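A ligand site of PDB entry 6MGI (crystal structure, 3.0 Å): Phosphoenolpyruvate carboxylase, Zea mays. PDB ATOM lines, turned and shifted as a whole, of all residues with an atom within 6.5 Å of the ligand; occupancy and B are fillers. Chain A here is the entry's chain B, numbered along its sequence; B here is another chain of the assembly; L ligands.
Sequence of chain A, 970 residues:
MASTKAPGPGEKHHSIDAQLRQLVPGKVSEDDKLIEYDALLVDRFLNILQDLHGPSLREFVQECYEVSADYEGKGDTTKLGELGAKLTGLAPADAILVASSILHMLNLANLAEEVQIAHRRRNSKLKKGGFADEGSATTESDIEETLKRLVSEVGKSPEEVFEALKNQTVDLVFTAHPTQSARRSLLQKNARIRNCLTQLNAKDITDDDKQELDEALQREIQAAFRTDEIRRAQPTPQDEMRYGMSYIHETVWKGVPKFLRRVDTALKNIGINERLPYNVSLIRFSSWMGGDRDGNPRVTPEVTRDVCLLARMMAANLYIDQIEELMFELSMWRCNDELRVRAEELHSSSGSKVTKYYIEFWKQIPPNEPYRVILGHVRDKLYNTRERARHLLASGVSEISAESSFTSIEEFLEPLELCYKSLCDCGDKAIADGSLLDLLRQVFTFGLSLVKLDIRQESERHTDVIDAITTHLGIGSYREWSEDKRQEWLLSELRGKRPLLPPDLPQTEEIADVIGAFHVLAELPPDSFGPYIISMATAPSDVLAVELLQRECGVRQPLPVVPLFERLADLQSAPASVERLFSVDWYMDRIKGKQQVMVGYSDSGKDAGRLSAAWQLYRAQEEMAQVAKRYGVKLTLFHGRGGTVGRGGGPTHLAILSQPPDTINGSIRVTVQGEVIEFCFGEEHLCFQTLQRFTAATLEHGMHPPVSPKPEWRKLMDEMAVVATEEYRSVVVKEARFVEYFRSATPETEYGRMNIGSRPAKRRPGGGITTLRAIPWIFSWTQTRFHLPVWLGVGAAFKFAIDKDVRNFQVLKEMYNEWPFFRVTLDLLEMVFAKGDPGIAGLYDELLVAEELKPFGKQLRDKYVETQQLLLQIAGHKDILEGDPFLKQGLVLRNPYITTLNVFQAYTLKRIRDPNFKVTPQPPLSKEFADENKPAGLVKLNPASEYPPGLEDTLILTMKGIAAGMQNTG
The backbone NH (N) of Arg 184 sits at hydrogen-bond distance from an oxygen (O8) of the ligand, 3.3 Å away.
The guanidinium group of Arg 231 lies within salt-bridge range of an oxygen (O8) of the ligand (2.5 Å).
An oxygen (O7) of the ligand is in salt-bridge range of the guanidinium group (NH2) of Arg 183 (2.9 Å).
The backbone NH of Ser 185 is in hydrogen-bond range of an oxygen (O9) of the ligand (3.0 Å).
NZ of Lys 363 of chain B is in hydrogen-bond range of O3 of the ligand, 3.0 Å away.
An oxygen (O2) of the ligand lies within hydrogen-bond range of the side-chain carboxylate (OD1) of Asp 239.
O1 of the ligand sits at hydrogen-bond distance from OE1 of Glu 360 of chain B (2.8 Å).
NE1 of Trp 362 of chain B lies close to O2 of the ligand, at 3.1 Å.
The backbone NH (N) of Phe 361 of chain B lies within hydrogen-bond range of an oxygen (O1) of the ligand (3.0 Å).
An oxygen (O9) of the ligand lies within hydrogen-bond range of the side-chain hydroxyl (OG) of Ser 185, 2.8 Å away.
NH2 of Arg 372 of chain B is in hydrogen-bond range of O of Phe 328 of chain B, at 3.0 Å.
NE1 of Trp 362 of chain B lies within hydrogen-bond range of OD1 of Asp 239 (2.5 Å).
The guanidinium group (NH2) of Arg 183 is in salt-bridge range of the side-chain carboxylate (OE2) of Glu 369 of chain B, 2.9 Å away.
The side-chain amino group (NZ) of Lys 363 of chain B lies within salt-bridge range of the side-chain carboxylate (OD2) of Asp 239, at 2.8 Å.
NH1 of Arg 372 of chain B is in salt-bridge range of OE2 of Glu 369 of chain B, at 3.4 Å.
The side-chain carboxylate of Glu 360 of chain B lies within salt-bridge range of the guanidinium group of Arg 184 (2.9 Å).
The side-chain hydroxyl (OG) of Ser 185 lies within hydrogen-bond range of the guanidinium group (NH2) of Arg 372 of chain B (2.5 Å).
Merely in contact with the ligand: Arg 372 of chain B.
Hydrophobic or aromatic side chains that line the ligand: Phe 361 of chain B and Trp 362 of chain B.
Ten residues have an atom within 4 Å of the ligand: Arg 183, Arg 184, Ser 185, Arg 231, Asp 239, Glu 360 of chain B, Phe 361 of chain B, Trp 362 of chain B, Lys 363 of chain B and Arg 372 of chain B.
The nearest printed residue that does not touch the ligand is Phe 328 of chain B (4.4 Å).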
ATOM      1  N   ALA A 182     -15.285  21.227   9.461  1.00  0.00           N
ATOM      2  CA  ALA A 182     -14.265  20.206   9.263  1.00  0.00           C
ATOM      3  C   ALA A 182     -14.777  18.832   9.680  1.00  0.00           C
ATOM      4  O   ALA A 182     -15.552  18.699  10.633  1.00  0.00           O
ATOM      5  CB  ALA A 182     -13.007  20.552  10.067  1.00  0.00           C
ATOM      6  N   ARG A 183     -14.345  17.813   8.945  1.00  0.00           N
ATOM      7  CA  ARG A 183     -14.648  16.439   9.305  1.00  0.00           C
ATOM      8  C   ARG A 183     -13.901  16.054  10.577  1.00  0.00           C
ATOM      9  O   ARG A 183     -12.830  16.583  10.885  1.00  0.00           O
ATOM     10  CB  ARG A 183     -14.266  15.486   8.177  1.00  0.00           C
ATOM     11  CG  ARG A 183     -15.121  15.567   6.931  1.00  0.00           C
ATOM     12  CD  ARG A 183     -14.768  14.446   5.963  1.00  0.00           C
ATOM     13  NE  ARG A 183     -15.007  13.135   6.552  1.00  0.00           N
ATOM     14  CZ  ARG A 183     -14.387  12.017   6.182  1.00  0.00           C
ATOM     15  NH1 ARG A 183     -13.473  12.057   5.223  1.00  0.00           N
ATOM     16  NH2 ARG A 183     -14.676  10.871   6.772  1.00  0.00           N
ATOM     17  N   ARG A 184     -14.485  15.098  11.320  1.00  0.00           N
ATOM     18  CA  ARG A 184     -13.834  14.612  12.531  1.00  0.00           C
ATOM     19  C   ARG A 184     -12.511  13.927  12.226  1.00  0.00           C
ATOM     20  O   ARG A 184     -11.579  13.996  13.034  1.00  0.00           O
ATOM     21  CB  ARG A 184     -14.762  13.668  13.286  1.00  0.00           C
ATOM     22  CG  ARG A 184     -15.796  14.383  14.142  1.00  0.00           C
ATOM     23  CD  ARG A 184     -16.532  13.417  15.030  1.00  0.00           C
ATOM     24  NE  ARG A 184     -15.630  12.699  15.932  1.00  0.00           N
ATOM     25  CZ  ARG A 184     -15.975  11.625  16.624  1.00  0.00           C
ATOM     26  NH1 ARG A 184     -17.194  11.123  16.515  1.00  0.00           N
ATOM     27  NH2 ARG A 184     -15.093  11.034  17.422  1.00  0.00           N
ATOM     28  N   SER A 185     -12.407  13.262  11.071  1.00  0.00           N
ATOM     29  CA  SER A 185     -11.141  12.664  10.677  1.00  0.00           C
ATOM     30  C   SER A 185     -10.066  13.736  10.498  1.00  0.00           C
ATOM     31  O   SER A 185      -8.889  13.498  10.798  1.00  0.00           O
ATOM     32  CB  SER A 185     -11.313  11.862   9.391  1.00  0.00           C
ATOM     33  OG  SER A 185     -12.192  10.764   9.581  1.00  0.00           O
ATOM     34  N   LEU A 186     -10.462  14.916  10.023  1.00  0.00           N
ATOM     35  CA  LEU A 186      -9.509  15.994   9.818  1.00  0.00           C
ATOM     36  C   LEU A 186      -9.149  16.664  11.142  1.00  0.00           C
ATOM     37  O   LEU A 186      -7.994  17.057  11.350  1.00  0.00           O
ATOM     38  CB  LEU A 186     -10.072  17.016   8.833  1.00  0.00           C
ATOM     39  CG  LEU A 186     -10.035  16.723   7.323  1.00  0.00           C
ATOM     40  CD1 LEU A 186     -10.318  15.270   6.967  1.00  0.00           C
ATOM     41  CD2 LEU A 186     -11.031  17.618   6.597  1.00  0.00           C
ATOM     42  N   ARG A 231     -17.833  15.737   3.411  1.00  0.00           N
ATOM     43  CA  ARG A 231     -18.682  14.743   4.066  1.00  0.00           C
ATOM     44  C   ARG A 231     -19.770  14.345   3.070  1.00  0.00           C
ATOM     45  O   ARG A 231     -20.741  15.078   2.877  1.00  0.00           O
ATOM     46  CB  ARG A 231     -19.265  15.300   5.353  1.00  0.00           C
ATOM     47  CG  ARG A 231     -19.217  14.321   6.529  1.00  0.00           C
ATOM     48  CD  ARG A 231     -20.306  14.604   7.534  1.00  0.00           C
ATOM     49  NE  ARG A 231     -20.029  15.794   8.341  1.00  0.00           N
ATOM     50  CZ  ARG A 231     -19.377  15.780   9.490  1.00  0.00           C
ATOM     51  NH1 ARG A 231     -18.921  14.635   9.988  1.00  0.00           N
ATOM     52  NH2 ARG A 231     -19.157  16.910  10.149  1.00  0.00           N
ATOM     53  N   GLN A 238     -27.264  11.243  16.245  1.00  0.00           N
ATOM     54  CA  GLN A 238     -26.427  10.404  17.093  1.00  0.00           C
ATOM     55  C   GLN A 238     -24.948  10.488  16.749  1.00  0.00           C
ATOM     56  O   GLN A 238     -24.121  10.047  17.557  1.00  0.00           O
ATOM     57  CB  GLN A 238     -26.902   8.951  17.005  1.00  0.00           C
ATOM     58  CG  GLN A 238     -28.305   8.729  17.552  1.00  0.00           C
ATOM     59  CD  GLN A 238     -29.305   8.359  16.476  1.00  0.00           C
ATOM     60  OE1 GLN A 238     -29.294   8.924  15.377  1.00  0.00           O
ATOM     61  NE2 GLN A 238     -30.169   7.396  16.783  1.00  0.00           N
ATOM     62  N   ASP A 239     -24.598  11.056  15.590  1.00  0.00           N
ATOM     63  CA  ASP A 239     -23.206  11.290  15.237  1.00  0.00           C
ATOM     64  C   ASP A 239     -22.695  12.633  15.764  1.00  0.00           C
ATOM     65  O   ASP A 239     -21.575  12.715  16.276  1.00  0.00           O
ATOM     66  CB  ASP A 239     -23.024  11.239  13.713  1.00  0.00           C
ATOM     67  CG  ASP A 239     -23.172   9.839  13.168  1.00  0.00           C
ATOM     68  OD1 ASP A 239     -22.697   8.891  13.812  1.00  0.00           O
ATOM     69  OD2 ASP A 239     -23.759   9.699  12.069  1.00  0.00           O
ATOM     70  N   ARG A 242     -21.763  12.102  19.078  1.00  0.00           N
ATOM     71  CA  ARG A 242     -20.416  11.539  19.160  1.00  0.00           C
ATOM     72  C   ARG A 242     -19.367  12.638  19.107  1.00  0.00           C
ATOM     73  O   ARG A 242     -18.416  12.640  19.897  1.00  0.00           O
ATOM     74  CB  ARG A 242     -20.180  10.546  18.011  1.00  0.00           C
ATOM     75  CG  ARG A 242     -21.186   9.433  17.910  1.00  0.00           C
ATOM     76  CD  ARG A 242     -20.770   8.282  18.792  1.00  0.00           C
ATOM     77  NE  ARG A 242     -21.347   7.006  18.366  1.00  0.00           N
ATOM     78  CZ  ARG A 242     -22.634   6.693  18.515  1.00  0.00           C
ATOM     79  NH1 ARG A 242     -23.465   7.562  19.061  1.00  0.00           N
ATOM     80  NH2 ARG A 242     -23.076   5.508  18.107  1.00  0.00           N
ATOM     81  N   PHE B 328      -9.630   5.169  12.808  1.00  0.00           N
ATOM     82  CA  PHE B 328      -9.852   6.604  12.722  1.00  0.00           C
ATOM     83  C   PHE B 328      -8.796   7.288  11.861  1.00  0.00           C
ATOM     84  O   PHE B 328      -9.082   8.326  11.253  1.00  0.00           O
ATOM     85  CB  PHE B 328      -9.855   7.201  14.128  1.00  0.00           C
ATOM     86  CG  PHE B 328     -10.966   8.177  14.363  1.00  0.00           C
ATOM     87  CD1 PHE B 328     -10.779   9.533  14.155  1.00  0.00           C
ATOM     88  CD2 PHE B 328     -12.204   7.736  14.797  1.00  0.00           C
ATOM     89  CE1 PHE B 328     -11.809  10.426  14.368  1.00  0.00           C
ATOM     90  CE2 PHE B 328     -13.233   8.628  15.020  1.00  0.00           C
ATOM     91  CZ  PHE B 328     -13.043   9.976  14.800  1.00  0.00           C
ATOM     92  N   SER B 331      -8.227   7.288   6.823  1.00  0.00           N
ATOM     93  CA  SER B 331      -9.435   7.789   6.195  1.00  0.00           C
ATOM     94  C   SER B 331      -9.236   8.072   4.702  1.00  0.00           C
ATOM     95  O   SER B 331     -10.043   8.780   4.098  1.00  0.00           O
ATOM     96  CB  SER B 331      -9.929   9.049   6.901  1.00  0.00           C
ATOM     97  OG  SER B 331      -8.866   9.949   7.135  1.00  0.00           O
ATOM     98  N   ILE B 359     -18.944   3.111  20.107  1.00  0.00           N
ATOM     99  CA  ILE B 359     -18.722   4.536  20.310  1.00  0.00           C
ATOM    100  C   ILE B 359     -18.251   5.209  19.020  1.00  0.00           C
ATOM    101  O   ILE B 359     -18.525   6.397  18.794  1.00  0.00           O
ATOM    102  CB  ILE B 359     -17.739   4.765  21.480  1.00  0.00           C
ATOM    103  CG1 ILE B 359     -18.463   4.494  22.798  1.00  0.00           C
ATOM    104  CG2 ILE B 359     -17.180   6.181  21.470  1.00  0.00           C
ATOM    105  CD1 ILE B 359     -17.754   5.046  24.016  1.00  0.00           C
ATOM    106  N   GLU B 360     -17.563   4.488  18.143  1.00  0.00           N
ATOM    107  CA  GLU B 360     -17.178   5.057  16.852  1.00  0.00           C
ATOM    108  C   GLU B 360     -17.408   4.028  15.752  1.00  0.00           C
ATOM    109  O   GLU B 360     -17.206   2.831  15.969  1.00  0.00           O
ATOM    110  CB  GLU B 360     -15.726   5.533  16.850  1.00  0.00           C
ATOM    111  CG  GLU B 360     -15.389   6.567  17.938  1.00  0.00           C
ATOM    112  CD  GLU B 360     -15.912   7.955  17.623  1.00  0.00           C
ATOM    113  OE1 GLU B 360     -15.917   8.338  16.432  1.00  0.00           O
ATOM    114  OE2 GLU B 360     -16.288   8.683  18.573  1.00  0.00           O
ATOM    115  N   PHE B 361     -17.829   4.510  14.584  1.00  0.00           N
ATOM    116  CA  PHE B 361     -18.106   3.667  13.418  1.00  0.00           C
ATOM    117  C   PHE B 361     -19.192   2.636  13.743  1.00  0.00           C
ATOM    118  O   PHE B 361     -19.003   1.412  13.634  1.00  0.00           O
ATOM    119  CB  PHE B 361     -16.829   3.002  12.904  1.00  0.00           C
ATOM    120  CG  PHE B 361     -15.726   3.988  12.644  1.00  0.00           C
ATOM    121  CD1 PHE B 361     -15.823   4.873  11.588  1.00  0.00           C
ATOM    122  CD2 PHE B 361     -14.611   4.037  13.455  1.00  0.00           C
ATOM    123  CE1 PHE B 361     -14.821   5.790  11.341  1.00  0.00           C
ATOM    124  CE2 PHE B 361     -13.604   4.945  13.217  1.00  0.00           C
ATOM    125  CZ  PHE B 361     -13.702   5.830  12.161  1.00  0.00           C
ATOM    126  N   TRP B 362     -20.340   3.163  14.155  1.00  0.00           N
ATOM    127  CA  TRP B 362     -21.479   2.349  14.569  1.00  0.00           C
ATOM    128  C   TRP B 362     -22.447   2.034  13.438  1.00  0.00           C
ATOM    129  O   TRP B 362     -23.240   1.092  13.575  1.00  0.00           O
ATOM    130  CB  TRP B 362     -22.240   3.071  15.690  1.00  0.00           C
ATOM    131  CG  TRP B 362     -22.802   4.381  15.255  1.00  0.00           C
ATOM    132  CD1 TRP B 362     -22.113   5.517  14.975  1.00  0.00           C
ATOM    133  CD2 TRP B 362     -24.187   4.688  15.062  1.00  0.00           C
ATOM    134  NE1 TRP B 362     -22.979   6.518  14.611  1.00  0.00           N
ATOM    135  CE2 TRP B 362     -24.254   6.037  14.658  1.00  0.00           C
ATOM    136  CE3 TRP B 362     -25.369   3.962  15.186  1.00  0.00           C
ATOM    137  CZ2 TRP B 362     -25.466   6.675  14.380  1.00  0.00           C
ATOM    138  CZ3 TRP B 362     -26.576   4.592  14.906  1.00  0.00           C
ATOM    139  CH2 TRP B 362     -26.607   5.933  14.511  1.00  0.00           C
ATOM    140  N   LYS B 363     -22.413   2.794  12.353  1.00  0.00           N
ATOM    141  CA  LYS B 363     -23.178   2.468  11.154  1.00  0.00           C
ATOM    142  C   LYS B 363     -22.299   1.690  10.185  1.00  0.00           C
ATOM    143  O   LYS B 363     -21.090   1.512  10.390  1.00  0.00           O
ATOM    144  CB  LYS B 363     -23.719   3.742  10.493  1.00  0.00           C
ATOM    145  CG  LYS B 363     -24.044   4.850  11.478  1.00  0.00           C
ATOM    146  CD  LYS B 363     -24.752   6.008  10.807  1.00  0.00           C
ATOM    147  CE  LYS B 363     -23.871   6.654   9.744  1.00  0.00           C
ATOM    148  NZ  LYS B 363     -22.996   7.713  10.295  1.00  0.00           N
ATOM    149  N   GLN B 364     -22.914   1.215   9.104  1.00  0.00           N
ATOM    150  CA  GLN B 364     -22.157   0.547   8.061  1.00  0.00           C
ATOM    151  C   GLN B 364     -21.161   1.525   7.439  1.00  0.00           C
ATOM    152  O   GLN B 364     -21.496   2.682   7.160  1.00  0.00           O
ATOM    153  CB  GLN B 364     -23.090  -0.003   6.990  1.00  0.00           C
ATOM    154  CG  GLN B 364     -22.396  -0.876   5.953  1.00  0.00           C
ATOM    155  CD  GLN B 364     -23.374  -1.553   5.019  1.00  0.00           C
ATOM    156  OE1 GLN B 364     -24.073  -0.886   4.256  1.00  0.00           O
ATOM    157  NE2 GLN B 364     -23.418  -2.879   5.066  1.00  0.00           N
ATOM    158  N   PRO B 366     -18.955   3.286   4.693  1.00  0.00           N
ATOM    159  CA  PRO B 366     -19.096   3.446   3.245  1.00  0.00           C
ATOM    160  C   PRO B 366     -17.905   2.838   2.520  1.00  0.00           C
ATOM    161  O   PRO B 366     -16.784   2.842   3.042  1.00  0.00           O
ATOM    162  CB  PRO B 366     -19.156   4.966   3.055  1.00  0.00           C
ATOM    163  CG  PRO B 366     -19.523   5.523   4.395  1.00  0.00           C
ATOM    164  CD  PRO B 366     -18.897   4.583   5.378  1.00  0.00           C
ATOM    165  N   GLU B 369     -14.375   4.568   1.839  1.00  0.00           N
ATOM    166  CA  GLU B 369     -13.370   4.580   2.890  1.00  0.00           C
ATOM    167  C   GLU B 369     -12.868   3.149   3.049  1.00  0.00           C
ATOM    168  O   GLU B 369     -13.188   2.475   4.032  1.00  0.00           O
ATOM    169  CB  GLU B 369     -13.930   5.133   4.196  1.00  0.00           C
ATOM    170  CG  GLU B 369     -14.509   6.536   4.076  1.00  0.00           C
ATOM    171  CD  GLU B 369     -15.130   7.029   5.376  1.00  0.00           C
ATOM    172  OE1 GLU B 369     -15.536   6.185   6.199  1.00  0.00           O
ATOM    173  OE2 GLU B 369     -15.214   8.256   5.562  1.00  0.00           O
ATOM    174  N   ARG B 372     -11.139   1.729   6.249  1.00  0.00           N
ATOM    175  CA  ARG B 372     -12.020   1.577   7.405  1.00  0.00           C
ATOM    176  C   ARG B 372     -12.916   0.365   7.248  1.00  0.00           C
ATOM    177  O   ARG B 372     -13.223  -0.315   8.241  1.00  0.00           O
ATOM    178  CB  ARG B 372     -12.835   2.851   7.619  1.00  0.00           C
ATOM    179  CG  ARG B 372     -11.961   4.086   7.779  1.00  0.00           C
ATOM    180  CD  ARG B 372     -12.784   5.327   8.049  1.00  0.00           C
ATOM    181  NE  ARG B 372     -12.039   6.295   8.845  1.00  0.00           N
ATOM    182  CZ  ARG B 372     -12.438   7.542   9.073  1.00  0.00           C
ATOM    183  NH1 ARG B 372     -13.569   7.986   8.546  1.00  0.00           N
ATOM    184  NH2 ARG B 372     -11.689   8.355   9.809  1.00  0.00           N
HETATM  185  C1  LIG L   1     -18.008   8.699  13.915  1.00  0.00           C
HETATM  186  C2  LIG L   1     -19.274   8.474  13.097  1.00  0.00           C
HETATM  187  C3  LIG L   1     -18.913   7.801  11.782  1.00  0.00           C
HETATM  188  C4  LIG L   1     -17.898   8.671  11.045  1.00  0.00           C
HETATM  189  C5  LIG L   1     -16.674   8.890  11.935  1.00  0.00           C
HETATM  190  C6  LIG L   1     -15.675   9.792  11.233  1.00  0.00           C
HETATM  191  O1  LIG L   1     -17.411   7.442  14.235  1.00  0.00           O
HETATM  192  O2  LIG L   1     -20.188   7.650  13.826  1.00  0.00           O
HETATM  193  O3  LIG L   1     -20.087   7.614  10.976  1.00  0.00           O
HETATM  194  O4  LIG L   1     -17.500   8.034   9.825  1.00  0.00           O
HETATM  195  O5  LIG L   1     -17.082   9.499  13.162  1.00  0.00           O
HETATM  196  O6  LIG L   1     -16.226  11.108  11.112  1.00  0.00           O
HETATM  197  P1  LIG L   1     -16.114  11.932   9.730  1.00  0.00           P
HETATM  198  O7  LIG L   1     -16.827  11.051   8.722  1.00  0.00           O
HETATM  199  O8  LIG L   1     -16.822  13.231  10.024  1.00  0.00           O
HETATM  200  O9  LIG L   1     -14.629  12.071   9.483  1.00  0.00           O
